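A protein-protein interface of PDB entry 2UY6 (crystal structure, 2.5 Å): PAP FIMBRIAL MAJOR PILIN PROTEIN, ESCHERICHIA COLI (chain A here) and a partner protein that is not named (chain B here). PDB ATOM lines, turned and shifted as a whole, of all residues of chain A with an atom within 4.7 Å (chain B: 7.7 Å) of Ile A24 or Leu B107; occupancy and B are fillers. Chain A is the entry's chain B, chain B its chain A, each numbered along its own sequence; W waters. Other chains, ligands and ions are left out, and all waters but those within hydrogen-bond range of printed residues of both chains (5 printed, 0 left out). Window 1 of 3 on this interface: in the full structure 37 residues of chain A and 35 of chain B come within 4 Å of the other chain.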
ATOM      1  N   CYS A  22      -7.785   4.050  10.652  1.00  0.00           N
ATOM      2  CA  CYS A  22      -8.137   4.913  11.767  1.00  0.00           C
ATOM      3  C   CYS A  22      -9.291   4.408  12.637  1.00  0.00           C
ATOM      4  O   CYS A  22     -10.190   3.705  12.175  1.00  0.00           O
ATOM      5  CB  CYS A  22      -8.453   6.324  11.265  1.00  0.00           C
ATOM      6  SG  CYS A  22      -6.993   7.240  10.680  1.00  0.00           S
ATOM      7  N   SER A  23      -9.231   4.772  13.912  1.00  0.00           N
ATOM      8  CA  SER A  23     -10.252   4.428  14.885  1.00  0.00           C
ATOM      9  C   SER A  23     -10.807   5.780  15.344  1.00  0.00           C
ATOM     10  O   SER A  23     -10.056   6.757  15.412  1.00  0.00           O
ATOM     11  CB  SER A  23      -9.616   3.684  16.061  1.00  0.00           C
ATOM     12  OG  SER A  23     -10.590   3.285  17.006  1.00  0.00           O
ATOM     13  N   ILE A  24     -12.102   5.873  15.636  1.00  0.00           N
ATOM     14  CA  ILE A  24     -12.637   7.165  16.088  1.00  0.00           C
ATOM     15  C   ILE A  24     -13.249   7.131  17.488  1.00  0.00           C
ATOM     16  O   ILE A  24     -13.593   6.070  18.017  1.00  0.00           O
ATOM     17  CB  ILE A  24     -13.709   7.760  15.105  1.00  0.00           C
ATOM     18  CG1 ILE A  24     -15.113   7.276  15.466  1.00  0.00           C
ATOM     19  CG2 ILE A  24     -13.386   7.389  13.675  1.00  0.00           C
ATOM     20  CD1 ILE A  24     -15.327   5.815  15.323  1.00  0.00           C
ATOM     21  N   SER A  25     -13.358   8.308  18.094  1.00  0.00           N
ATOM     22  CA  SER A  25     -13.964   8.437  19.412  1.00  0.00           C
ATOM     23  C   SER A  25     -14.384   9.884  19.651  1.00  0.00           C
ATOM     24  O   SER A  25     -13.950  10.792  18.943  1.00  0.00           O
ATOM     25  CB  SER A  25     -12.993   7.976  20.500  1.00  0.00           C
ATOM     26  OG  SER A  25     -11.806   8.731  20.462  1.00  0.00           O
ATOM     27  N   GLN A  31     -20.616   8.002  21.649  1.00  0.00           N
ATOM     28  CA  GLN A  31     -20.455   8.721  20.389  1.00  0.00           C
ATOM     29  C   GLN A  31     -21.726   9.440  19.927  1.00  0.00           C
ATOM     30  O   GLN A  31     -22.254   9.222  18.839  1.00  0.00           O
ATOM     31  CB  GLN A  31     -19.932   7.748  19.318  1.00  0.00           C
ATOM     32  CG  GLN A  31     -18.597   7.111  19.727  1.00  0.00           C
ATOM     33  CD  GLN A  31     -18.022   6.147  18.689  1.00  0.00           C
ATOM     34  OE1 GLN A  31     -18.684   5.793  17.705  1.00  0.00           O
ATOM     35  NE2 GLN A  31     -16.785   5.712  18.914  1.00  0.00           N
ATOM     36  N   ILE A  56     -14.749  14.538  15.924  1.00  0.00           N
ATOM     37  CA  ILE A  56     -14.373  13.142  15.782  1.00  0.00           C
ATOM     38  C   ILE A  56     -12.862  13.004  15.890  1.00  0.00           C
ATOM     39  O   ILE A  56     -12.126  13.516  15.048  1.00  0.00           O
ATOM     40  CB  ILE A  56     -14.826  12.581  14.414  1.00  0.00           C
ATOM     41  CG1 ILE A  56     -16.336  12.746  14.261  1.00  0.00           C
ATOM     42  CG2 ILE A  56     -14.467  11.111  14.305  1.00  0.00           C
ATOM     43  CD1 ILE A  56     -16.848  12.379  12.879  1.00  0.00           C
ATOM     44  N   GLU A  57     -12.401  12.324  16.936  1.00  0.00           N
ATOM     45  CA  GLU A  57     -10.974  12.126  17.132  1.00  0.00           C
ATOM     46  C   GLU A  57     -10.475  10.869  16.415  1.00  0.00           C
ATOM     47  O   GLU A  57     -10.979   9.769  16.644  1.00  0.00           O
ATOM     48  CB  GLU A  57     -10.645  12.052  18.632  1.00  0.00           C
ATOM     49  CG  GLU A  57      -9.234  11.528  18.929  1.00  0.00           C
ATOM     50  CD  GLU A  57      -8.725  11.872  20.329  1.00  0.00           C
ATOM     51  OE1 GLU A  57      -9.495  11.749  21.310  1.00  0.00           O
ATOM     52  OE2 GLU A  57      -7.541  12.253  20.447  1.00  0.00           O
ATOM     53  N   LEU A  58      -9.499  11.062  15.530  1.00  0.00           N
ATOM     54  CA  LEU A  58      -8.887   9.970  14.774  1.00  0.00           C
ATOM     55  C   LEU A  58      -7.721   9.427  15.590  1.00  0.00           C
ATOM     56  O   LEU A  58      -6.751  10.139  15.829  1.00  0.00           O
ATOM     57  CB  LEU A  58      -8.373  10.477  13.422  1.00  0.00           C
ATOM     58  CG  LEU A  58      -9.466  11.089  12.542  1.00  0.00           C
ATOM     59  CD1 LEU A  58      -8.887  11.660  11.249  1.00  0.00           C
ATOM     60  CD2 LEU A  58     -10.488  10.024  12.240  1.00  0.00           C
ATOM     61  N   VAL A  59      -7.819   8.174  16.027  1.00  0.00           N
ATOM     62  CA  VAL A  59      -6.753   7.567  16.823  1.00  0.00           C
ATOM     63  C   VAL A  59      -6.210   6.259  16.243  1.00  0.00           C
ATOM     64  O   VAL A  59      -6.747   5.713  15.277  1.00  0.00           O
ATOM     65  CB  VAL A  59      -7.228   7.300  18.267  1.00  0.00           C
ATOM     66  CG1 VAL A  59      -7.646   8.601  18.914  1.00  0.00           C
ATOM     67  CG2 VAL A  59      -8.393   6.310  18.269  1.00  0.00           C
ATOM     68  N   PHE A 158     -20.195   7.203   9.558  1.00  0.00           N
ATOM     69  CA  PHE A 158     -18.971   7.881   9.161  1.00  0.00           C
ATOM     70  C   PHE A 158     -18.151   6.813   8.451  1.00  0.00           C
ATOM     71  O   PHE A 158     -17.570   5.936   9.092  1.00  0.00           O
ATOM     72  CB  PHE A 158     -18.228   8.386  10.397  1.00  0.00           C
ATOM     73  CG  PHE A 158     -17.008   9.203  10.084  1.00  0.00           C
ATOM     74  CD1 PHE A 158     -17.104  10.358   9.317  1.00  0.00           C
ATOM     75  CD2 PHE A 158     -15.765   8.828  10.570  1.00  0.00           C
ATOM     76  CE1 PHE A 158     -15.973  11.131   9.041  1.00  0.00           C
ATOM     77  CE2 PHE A 158     -14.631   9.595  10.301  1.00  0.00           C
ATOM     78  CZ  PHE A 158     -14.736  10.749   9.535  1.00  0.00           C
ATOM     79  N   LEU A 160     -15.019   5.482   6.181  1.00  0.00           N
ATOM     80  CA  LEU A 160     -13.638   5.683   5.748  1.00  0.00           C
ATOM     81  C   LEU A 160     -13.274   4.525   4.822  1.00  0.00           C
ATOM     82  O   LEU A 160     -13.211   3.368   5.256  1.00  0.00           O
ATOM     83  CB  LEU A 160     -12.694   5.691   6.953  1.00  0.00           C
ATOM     84  CG  LEU A 160     -12.948   6.808   7.966  1.00  0.00           C
ATOM     85  CD1 LEU A 160     -11.923   6.748   9.092  1.00  0.00           C
ATOM     86  CD2 LEU A 160     -12.884   8.148   7.244  1.00  0.00           C
ATOM     87  N   ALA B   1     -15.500   3.467  17.736  1.00  0.00           N
ATOM     88  CA  ALA B   1     -14.928   2.668  18.868  1.00  0.00           C
ATOM     89  C   ALA B   1     -14.291   1.351  18.396  1.00  0.00           C
ATOM     90  O   ALA B   1     -13.274   0.928  18.938  1.00  0.00           O
ATOM     91  CB  ALA B   1     -16.011   2.391  19.906  1.00  0.00           C
ATOM     92  N   VAL B   2     -14.890   0.715  17.390  1.00  0.00           N
ATOM     93  CA  VAL B   2     -14.389  -0.538  16.833  1.00  0.00           C
ATOM     94  C   VAL B   2     -13.394  -0.271  15.693  1.00  0.00           C
ATOM     95  O   VAL B   2     -13.643   0.575  14.827  1.00  0.00           O
ATOM     96  CB  VAL B   2     -15.554  -1.387  16.294  1.00  0.00           C
ATOM     97  CG1 VAL B   2     -15.026  -2.678  15.669  1.00  0.00           C
ATOM     98  CG2 VAL B   2     -16.533  -1.688  17.427  1.00  0.00           C
ATOM     99  N   SER B   3     -12.285  -1.008  15.680  1.00  0.00           N
ATOM    100  CA  SER B   3     -11.249  -0.817  14.660  1.00  0.00           C
ATOM    101  C   SER B   3     -10.713  -2.098  14.006  1.00  0.00           C
ATOM    102  O   SER B   3     -10.790  -3.188  14.582  1.00  0.00           O
ATOM    103  CB  SER B   3     -10.071  -0.035  15.258  1.00  0.00           C
ATOM    104  OG  SER B   3      -9.499  -0.724  16.365  1.00  0.00           O
ATOM    105  N   LEU B   4     -10.163  -1.939  12.802  1.00  0.00           N
ATOM    106  CA  LEU B   4      -9.592  -3.030  12.006  1.00  0.00           C
ATOM    107  C   LEU B   4      -8.069  -2.968  12.160  1.00  0.00           C
ATOM    108  O   LEU B   4      -7.532  -1.930  12.570  1.00  0.00           O
ATOM    109  CB  LEU B   4      -9.946  -2.845  10.533  1.00  0.00           C
ATOM    110  CG  LEU B   4     -10.508  -4.012   9.724  1.00  0.00           C
ATOM    111  CD1 LEU B   4     -10.139  -3.810   8.266  1.00  0.00           C
ATOM    112  CD2 LEU B   4      -9.985  -5.328  10.234  1.00  0.00           C
ATOM    113  N   ASP B  25     -11.858  -0.259  20.863  1.00  0.00           N
ATOM    114  CA  ASP B  25     -10.970   0.654  21.556  1.00  0.00           C
ATOM    115  C   ASP B  25     -11.675   1.467  22.639  1.00  0.00           C
ATOM    116  O   ASP B  25     -11.040   2.231  23.364  1.00  0.00           O
ATOM    117  CB  ASP B  25     -10.276   1.574  20.551  1.00  0.00           C
ATOM    118  CG  ASP B  25      -9.447   0.802  19.524  1.00  0.00           C
ATOM    119  OD1 ASP B  25      -8.750  -0.165  19.915  1.00  0.00           O
ATOM    120  OD2 ASP B  25      -9.485   1.170  18.329  1.00  0.00           O
ATOM    121  N   ASN B  26     -12.984   1.298  22.762  1.00  0.00           N
ATOM    122  CA  ASN B  26     -13.718   2.019  23.787  1.00  0.00           C
ATOM    123  C   ASN B  26     -13.645   1.197  25.075  1.00  0.00           C
ATOM    124  O   ASN B  26     -14.078   0.041  25.113  1.00  0.00           O
ATOM    125  CB  ASN B  26     -15.170   2.209  23.362  1.00  0.00           C
ATOM    126  CG  ASN B  26     -15.913   3.187  24.251  1.00  0.00           C
ATOM    127  OD1 ASN B  26     -16.367   4.231  23.793  1.00  0.00           O
ATOM    128  ND2 ASN B  26     -16.038   2.853  25.528  1.00  0.00           N
ATOM    129  N   TYR B  31     -19.716  -2.275  22.147  1.00  0.00           N
ATOM    130  CA  TYR B  31     -20.163  -1.892  20.820  1.00  0.00           C
ATOM    131  C   TYR B  31     -20.303  -3.161  20.005  1.00  0.00           C
ATOM    132  O   TYR B  31     -19.626  -4.155  20.269  1.00  0.00           O
ATOM    133  CB  TYR B  31     -19.138  -0.985  20.132  1.00  0.00           C
ATOM    134  CG  TYR B  31     -19.208   0.478  20.494  1.00  0.00           C
ATOM    135  CD1 TYR B  31     -18.869   0.922  21.766  1.00  0.00           C
ATOM    136  CD2 TYR B  31     -19.577   1.424  19.541  1.00  0.00           C
ATOM    137  CE1 TYR B  31     -18.892   2.280  22.084  1.00  0.00           C
ATOM    138  CE2 TYR B  31     -19.602   2.775  19.842  1.00  0.00           C
ATOM    139  CZ  TYR B  31     -19.262   3.203  21.114  1.00  0.00           C
ATOM    140  OH  TYR B  31     -19.319   4.552  21.411  1.00  0.00           O
ATOM    141  N   LEU B  32     -21.186  -3.133  19.016  1.00  0.00           N
ATOM    142  CA  LEU B  32     -21.358  -4.283  18.156  1.00  0.00           C
ATOM    143  C   LEU B  32     -20.492  -4.008  16.944  1.00  0.00           C
ATOM    144  O   LEU B  32     -20.231  -2.850  16.615  1.00  0.00           O
ATOM    145  CB  LEU B  32     -22.816  -4.437  17.725  1.00  0.00           C
ATOM    146  CG  LEU B  32     -23.843  -4.702  18.829  1.00  0.00           C
ATOM    147  CD1 LEU B  32     -25.196  -5.031  18.210  1.00  0.00           C
ATOM    148  CD2 LEU B  32     -23.361  -5.857  19.703  1.00  0.00           C
ATOM    149  N   GLN B  34     -20.218  -5.257  12.915  1.00  0.00           N
ATOM    150  CA  GLN B  34     -20.773  -6.010  11.793  1.00  0.00           C
ATOM    151  C   GLN B  34     -19.677  -6.127  10.761  1.00  0.00           C
ATOM    152  O   GLN B  34     -18.845  -5.224  10.629  1.00  0.00           O
ATOM    153  CB  GLN B  34     -21.927  -5.276  11.134  1.00  0.00           C
ATOM    154  CG  GLN B  34     -22.877  -4.582  12.072  1.00  0.00           C
ATOM    155  CD  GLN B  34     -24.048  -3.984  11.323  1.00  0.00           C
ATOM    156  OE1 GLN B  34     -25.028  -4.665  11.064  1.00  0.00           O
ATOM    157  NE2 GLN B  34     -23.936  -2.710  10.944  1.00  0.00           N
ATOM    158  N   LEU B  90     -16.212  -3.331   7.945  1.00  0.00           N
ATOM    159  CA  LEU B  90     -16.370  -3.473   9.384  1.00  0.00           C
ATOM    160  C   LEU B  90     -17.088  -2.201   9.840  1.00  0.00           C
ATOM    161  O   LEU B  90     -16.560  -1.097   9.710  1.00  0.00           O
ATOM    162  CB  LEU B  90     -15.018  -3.588  10.081  1.00  0.00           C
ATOM    163  CG  LEU B  90     -15.067  -3.872  11.589  1.00  0.00           C
ATOM    164  CD1 LEU B  90     -15.472  -5.334  11.827  1.00  0.00           C
ATOM    165  CD2 LEU B  90     -13.701  -3.597  12.225  1.00  0.00           C
ATOM    166  N   ARG B  91     -18.307  -2.352  10.343  1.00  0.00           N
ATOM    167  CA  ARG B  91     -19.073  -1.199  10.807  1.00  0.00           C
ATOM    168  C   ARG B  91     -19.624  -1.459  12.200  1.00  0.00           C
ATOM    169  O   ARG B  91     -20.187  -2.520  12.457  1.00  0.00           O
ATOM    170  CB  ARG B  91     -20.234  -0.900   9.864  1.00  0.00           C
ATOM    171  CG  ARG B  91     -21.179   0.131  10.447  1.00  0.00           C
ATOM    172  CD  ARG B  91     -22.594  -0.143  10.054  1.00  0.00           C
ATOM    173  NE  ARG B  91     -22.816   0.232   8.675  1.00  0.00           N
ATOM    174  CZ  ARG B  91     -23.749  -0.308   7.906  1.00  0.00           C
ATOM    175  NH1 ARG B  91     -23.887   0.105   6.649  1.00  0.00           N
ATOM    176  NH2 ARG B  91     -24.529  -1.275   8.387  1.00  0.00           N
ATOM    177  N   GLU B  92     -19.476  -0.484  13.089  1.00  0.00           N
ATOM    178  CA  GLU B  92     -19.945  -0.619  14.462  1.00  0.00           C
ATOM    179  C   GLU B  92     -21.387  -0.160  14.673  1.00  0.00           C
ATOM    180  O   GLU B  92     -21.954   0.588  13.868  1.00  0.00           O
ATOM    181  CB  GLU B  92     -19.041   0.182  15.405  1.00  0.00           C
ATOM    182  CG  GLU B  92     -19.131   1.694  15.200  1.00  0.00           C
ATOM    183  CD  GLU B  92     -18.056   2.474  15.953  1.00  0.00           C
ATOM    184  OE1 GLU B  92     -17.953   3.700  15.713  1.00  0.00           O
ATOM    185  OE2 GLU B  92     -17.320   1.869  16.779  1.00  0.00           O
ATOM    186  N   ILE B  93     -21.975  -0.636  15.763  1.00  0.00           N
ATOM    187  CA  ILE B  93     -23.324  -0.250  16.147  1.00  0.00           C
ATOM    188  C   ILE B  93     -23.154   0.261  17.571  1.00  0.00           C
ATOM    189  O   ILE B  93     -23.070  -0.526  18.515  1.00  0.00           O
ATOM    190  CB  ILE B  93     -24.299  -1.437  16.180  1.00  0.00           C
ATOM    191  CG1 ILE B  93     -24.430  -2.065  14.793  1.00  0.00           C
ATOM    192  CG2 ILE B  93     -25.663  -0.957  16.672  1.00  0.00           C
ATOM    193  CD1 ILE B  93     -25.078  -1.166  13.772  1.00  0.00           C
ATOM    194  N   PRO B  94     -23.076   1.585  17.747  1.00  0.00           N
ATOM    195  CA  PRO B  94     -22.908   2.106  19.108  1.00  0.00           C
ATOM    196  C   PRO B  94     -24.133   1.796  19.955  1.00  0.00           C
ATOM    197  O   PRO B  94     -25.234   1.643  19.431  1.00  0.00           O
ATOM    198  CB  PRO B  94     -22.702   3.600  18.878  1.00  0.00           C
ATOM    199  CG  PRO B  94     -23.554   3.862  17.678  1.00  0.00           C
ATOM    200  CD  PRO B  94     -23.289   2.676  16.780  1.00  0.00           C
ATOM    201  N   GLN B 104     -25.903  10.206  16.809  1.00  0.00           N
ATOM    202  CA  GLN B 104     -24.774   9.328  17.080  1.00  0.00           C
ATOM    203  C   GLN B 104     -23.980   9.024  15.807  1.00  0.00           C
ATOM    204  O   GLN B 104     -24.543   8.915  14.712  1.00  0.00           O
ATOM    205  CB  GLN B 104     -25.242   8.021  17.726  1.00  0.00           C
ATOM    206  CG  GLN B 104     -25.998   8.221  19.018  1.00  0.00           C
ATOM    207  CD  GLN B 104     -26.336   6.921  19.713  1.00  0.00           C
ATOM    208  OE1 GLN B 104     -25.485   6.316  20.360  1.00  0.00           O
ATOM    209  NE2 GLN B 104     -27.587   6.480  19.579  1.00  0.00           N
ATOM    210  N   ILE B 105     -22.664   8.901  15.962  1.00  0.00           N
ATOM    211  CA  ILE B 105     -21.765   8.594  14.854  1.00  0.00           C
ATOM    212  C   ILE B 105     -21.334   7.122  14.900  1.00  0.00           C
ATOM    213  O   ILE B 105     -20.951   6.607  15.954  1.00  0.00           O
ATOM    214  CB  ILE B 105     -20.504   9.484  14.915  1.00  0.00           C
ATOM    215  CG1 ILE B 105     -20.892  10.950  14.723  1.00  0.00           C
ATOM    216  CG2 ILE B 105     -19.497   9.054  13.853  1.00  0.00           C
ATOM    217  CD1 ILE B 105     -21.692  11.218  13.466  1.00  0.00           C
ATOM    218  N   ALA B 106     -21.390   6.450  13.755  1.00  0.00           N
ATOM    219  CA  ALA B 106     -21.001   5.041  13.671  1.00  0.00           C
ATOM    220  C   ALA B 106     -19.939   4.885  12.590  1.00  0.00           C
ATOM    221  O   ALA B 106     -20.182   5.210  11.429  1.00  0.00           O
ATOM    222  CB  ALA B 106     -22.219   4.178  13.344  1.00  0.00           C
ATOM    223  N   LEU B 107     -18.774   4.376  12.970  1.00  0.00           N
ATOM    224  CA  LEU B 107     -17.672   4.208  12.022  1.00  0.00           C
ATOM    225  C   LEU B 107     -17.749   2.957  11.174  1.00  0.00           C
ATOM    226  O   LEU B 107     -18.006   1.863  11.677  1.00  0.00           O
ATOM    227  CB  LEU B 107     -16.330   4.197  12.764  1.00  0.00           C
ATOM    228  CG  LEU B 107     -14.962   4.319  12.060  1.00  0.00           C
ATOM    229  CD1 LEU B 107     -14.170   3.045  12.261  1.00  0.00           C
ATOM    230  CD2 LEU B 107     -15.114   4.651  10.578  1.00  0.00           C
ATOM    231  N   GLN B 108     -17.540   3.131   9.877  1.00  0.00           N
ATOM    232  CA  GLN B 108     -17.502   2.007   8.962  1.00  0.00           C
ATOM    233  C   GLN B 108     -16.159   2.085   8.264  1.00  0.00           C
ATOM    234  O   GLN B 108     -15.840   3.104   7.647  1.00  0.00           O
ATOM    235  CB  GLN B 108     -18.601   2.064   7.899  1.00  0.00           C
ATOM    236  CG  GLN B 108     -18.404   0.985   6.842  1.00  0.00           C
ATOM    237  CD  GLN B 108     -19.512   0.929   5.819  1.00  0.00           C
ATOM    238  OE1 GLN B 108     -20.687   0.883   6.170  1.00  0.00           O
ATOM    239  NE2 GLN B 108     -19.144   0.907   4.544  1.00  0.00           N
ATOM    240  N   THR B 109     -15.383   1.013   8.379  1.00  0.00           N
ATOM    241  CA  THR B 109     -14.070   0.903   7.748  1.00  0.00           C
ATOM    242  C   THR B 109     -14.204  -0.018   6.552  1.00  0.00           C
ATOM    243  O   THR B 109     -14.619  -1.167   6.700  1.00  0.00           O
ATOM    244  CB  THR B 109     -13.054   0.273   8.704  1.00  0.00           C
ATOM    245  OG1 THR B 109     -12.854   1.149   9.816  1.00  0.00           O
ATOM    246  CG2 THR B 109     -11.732   0.009   8.005  1.00  0.00           C
ATOM    247  N   LYS B 110     -13.871   0.476   5.369  1.00  0.00           N
ATOM    248  CA  LYS B 110     -13.949  -0.359   4.179  1.00  0.00           C
ATOM    249  C   LYS B 110     -12.552  -0.479   3.602  1.00  0.00           C
ATOM    250  O   LYS B 110     -11.872   0.533   3.422  1.00  0.00           O
ATOM    251  CB  LYS B 110     -14.858   0.261   3.125  1.00  0.00           C
ATOM    252  CG  LYS B 110     -15.147  -0.669   1.953  1.00  0.00           C
ATOM    253  CD  LYS B 110     -15.426   0.126   0.699  1.00  0.00           C
ATOM    254  CE  LYS B 110     -16.744  -0.253   0.055  1.00  0.00           C
ATOM    255  NZ  LYS B 110     -17.910   0.170   0.870  1.00  0.00           N
HETATM  256  O   HOH W   1     -15.906   5.233  21.251  1.00  0.00           O
HETATM  257  O   HOH W   2     -10.678   0.717  11.663  1.00  0.00           O
HETATM  258  O   HOH W   3     -13.127   3.089  15.940  1.00  0.00           O
HETATM  259  O   HOH W   4     -11.100   3.505   9.713  1.00  0.00           O
HETATM  260  O   HOH W   5     -16.715   3.273   4.318  1.00  0.00           O
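Ser A23 touches just these residues of chain B: Ser B3 (3.8 Å) and Asp B25 (2.7 Å).
Ile A24 touches just these residues of chain B: Ala B1, Glu B92 and Leu B107.
Of the printed residues of chain B, Gln A31 touches Ala B1, Tyr B31, Glu B92, Gln B104 and Ile B105.
Ile A56 touches none of the printed residues of chain B.
Of the printed residues of chain B, Phe A158 touches Ile B105 (3.7 Å), Ala B106 (2.7 Å), Leu B107 (3.1 Å) and Gln B108 (2.9 Å).
Of the printed residues of chain A, Ser B3 touches Ser A23 (3.8 Å).
Printed residues of chain A within 4 Å of Asp B25: Ser A23.
Of chain A, only Ile A24 and Phe A158 come within 4 Å of Leu B107.
The nearest residue of chain B that does not touch Ile A24 is Ile B105 (5.0 Å).
The nearest printed residue of chain A that does not touch Leu B107 is Leu A160 (4.02 Å).
The nearest printed residue of chain B that does not touch Gln A31 is Ala B106 (4.7 Å).
Of the 11 printed residues of chain A, 5 touch a printed residue of chain B.
Hydrophobic or aromatic side chains of chain A within 4 Å of the printed part of chain B: Ile A24 and Phe A158.
Water W1 lies within hydrogen-bond range of the side-chain amide nitrogen of Gln A31 (2.5 Å), the side-chain amide oxygen of Asn B26 (2.8 Å) and the side-chain hydroxyl of Tyr B31 (3.5 Å).
Water W4 lies within hydrogen-bond range of the backbone carbonyl oxygen (O) of Cys A22 (2.6 Å) and the side-chain hydroxyl (OG1) of Thr B109 (2.9 Å).
Water W3 lies within hydrogen-bond range of OG of Ser A23, O of Val B2, N of Ile A24 and N of Ala B1.
Water W2 lies within hydrogen-bond range of the side-chain hydroxyl (OG1) of Thr B109 (2.9 Å), the backbone NH (N) of Leu B4 (2.9 Å) and the backbone carbonyl oxygen (O) of Cys A22 (3.1 Å).
Water W5 bridges N of Leu A160 and NE2 of Gln B108.
Ser B3 touches Ser A23 (CB to OG, 3.8 Å).
Glu B92 touches Ile A24.
Ile A24 touches Leu B107.
Tyr B31 touches Gln A31.
Gln B104 touches Gln A31.
CG2 of Ile B105 touches CB of Phe A158 (3.7 Å).
CD2 of Leu B107 touches O of Phe A158 (3.1 Å).
CA of Thr B109 touches O of Leu A160, at 3.6 Å.
The backbone carbonyl oxygen of Ala B1 sits at hydrogen-bond distance from the backbone NH of Asp B25, 2.7 Å away.
N of Ala B1 sits at hydrogen-bond distance from OE2 of Glu B92 (2.6 Å).
The side-chain carboxylate of Glu B92 sits at hydrogen-bond distance from the backbone NH of Val B2 (2.8 Å).
The side-chain hydroxyl of Ser B3 sits at hydrogen-bond distance from the side-chain carboxylate of Asp B25, at 2.7 Å.
The side-chain carboxylate (OE1) of Glu B92 sits at hydrogen-bond distance from the backbone NH (N) of Leu B107 (2.9 Å).
O of Ile A24 sits at hydrogen-bond distance from NE2 of Gln A31 (3.3 Å).
The backbone NH of Ala B1 sits at hydrogen-bond distance from the backbone carbonyl oxygen of Ile A24, at 3.2 Å.
The side-chain amide nitrogen of Gln A31 sits close to the backbone NH of Ala B1.
The side-chain carboxylate (OD2) of Asp B25 is in hydrogen-bond range of the side-chain hydroxyl (OG) of Ser A23 (2.7 Å).
OE1 of Gln A31 lies close to OE1 of Glu B92 (3.0 Å).
The backbone NH (N) of Ile B105 is in hydrogen-bond range of the backbone carbonyl oxygen (O) of Gln A31 (2.9 Å).
The backbone carbonyl oxygen (O) of Ala B106 lies within hydrogen-bond range of the backbone NH (N) of Phe A158 (2.7 Å).
The backbone NH (N) of Gln B108 is in hydrogen-bond range of the backbone carbonyl oxygen (O) of Phe A158 (2.9 Å).
The backbone carbonyl oxygen (O) of Gln B108 lies within hydrogen-bond range of the backbone NH (N) of Leu A160, at 2.9 Å.
The backbone carbonyl oxygen (O) of Leu A160 lies within hydrogen-bond range of the backbone NH (N) of Lys B110 (3.0 Å).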
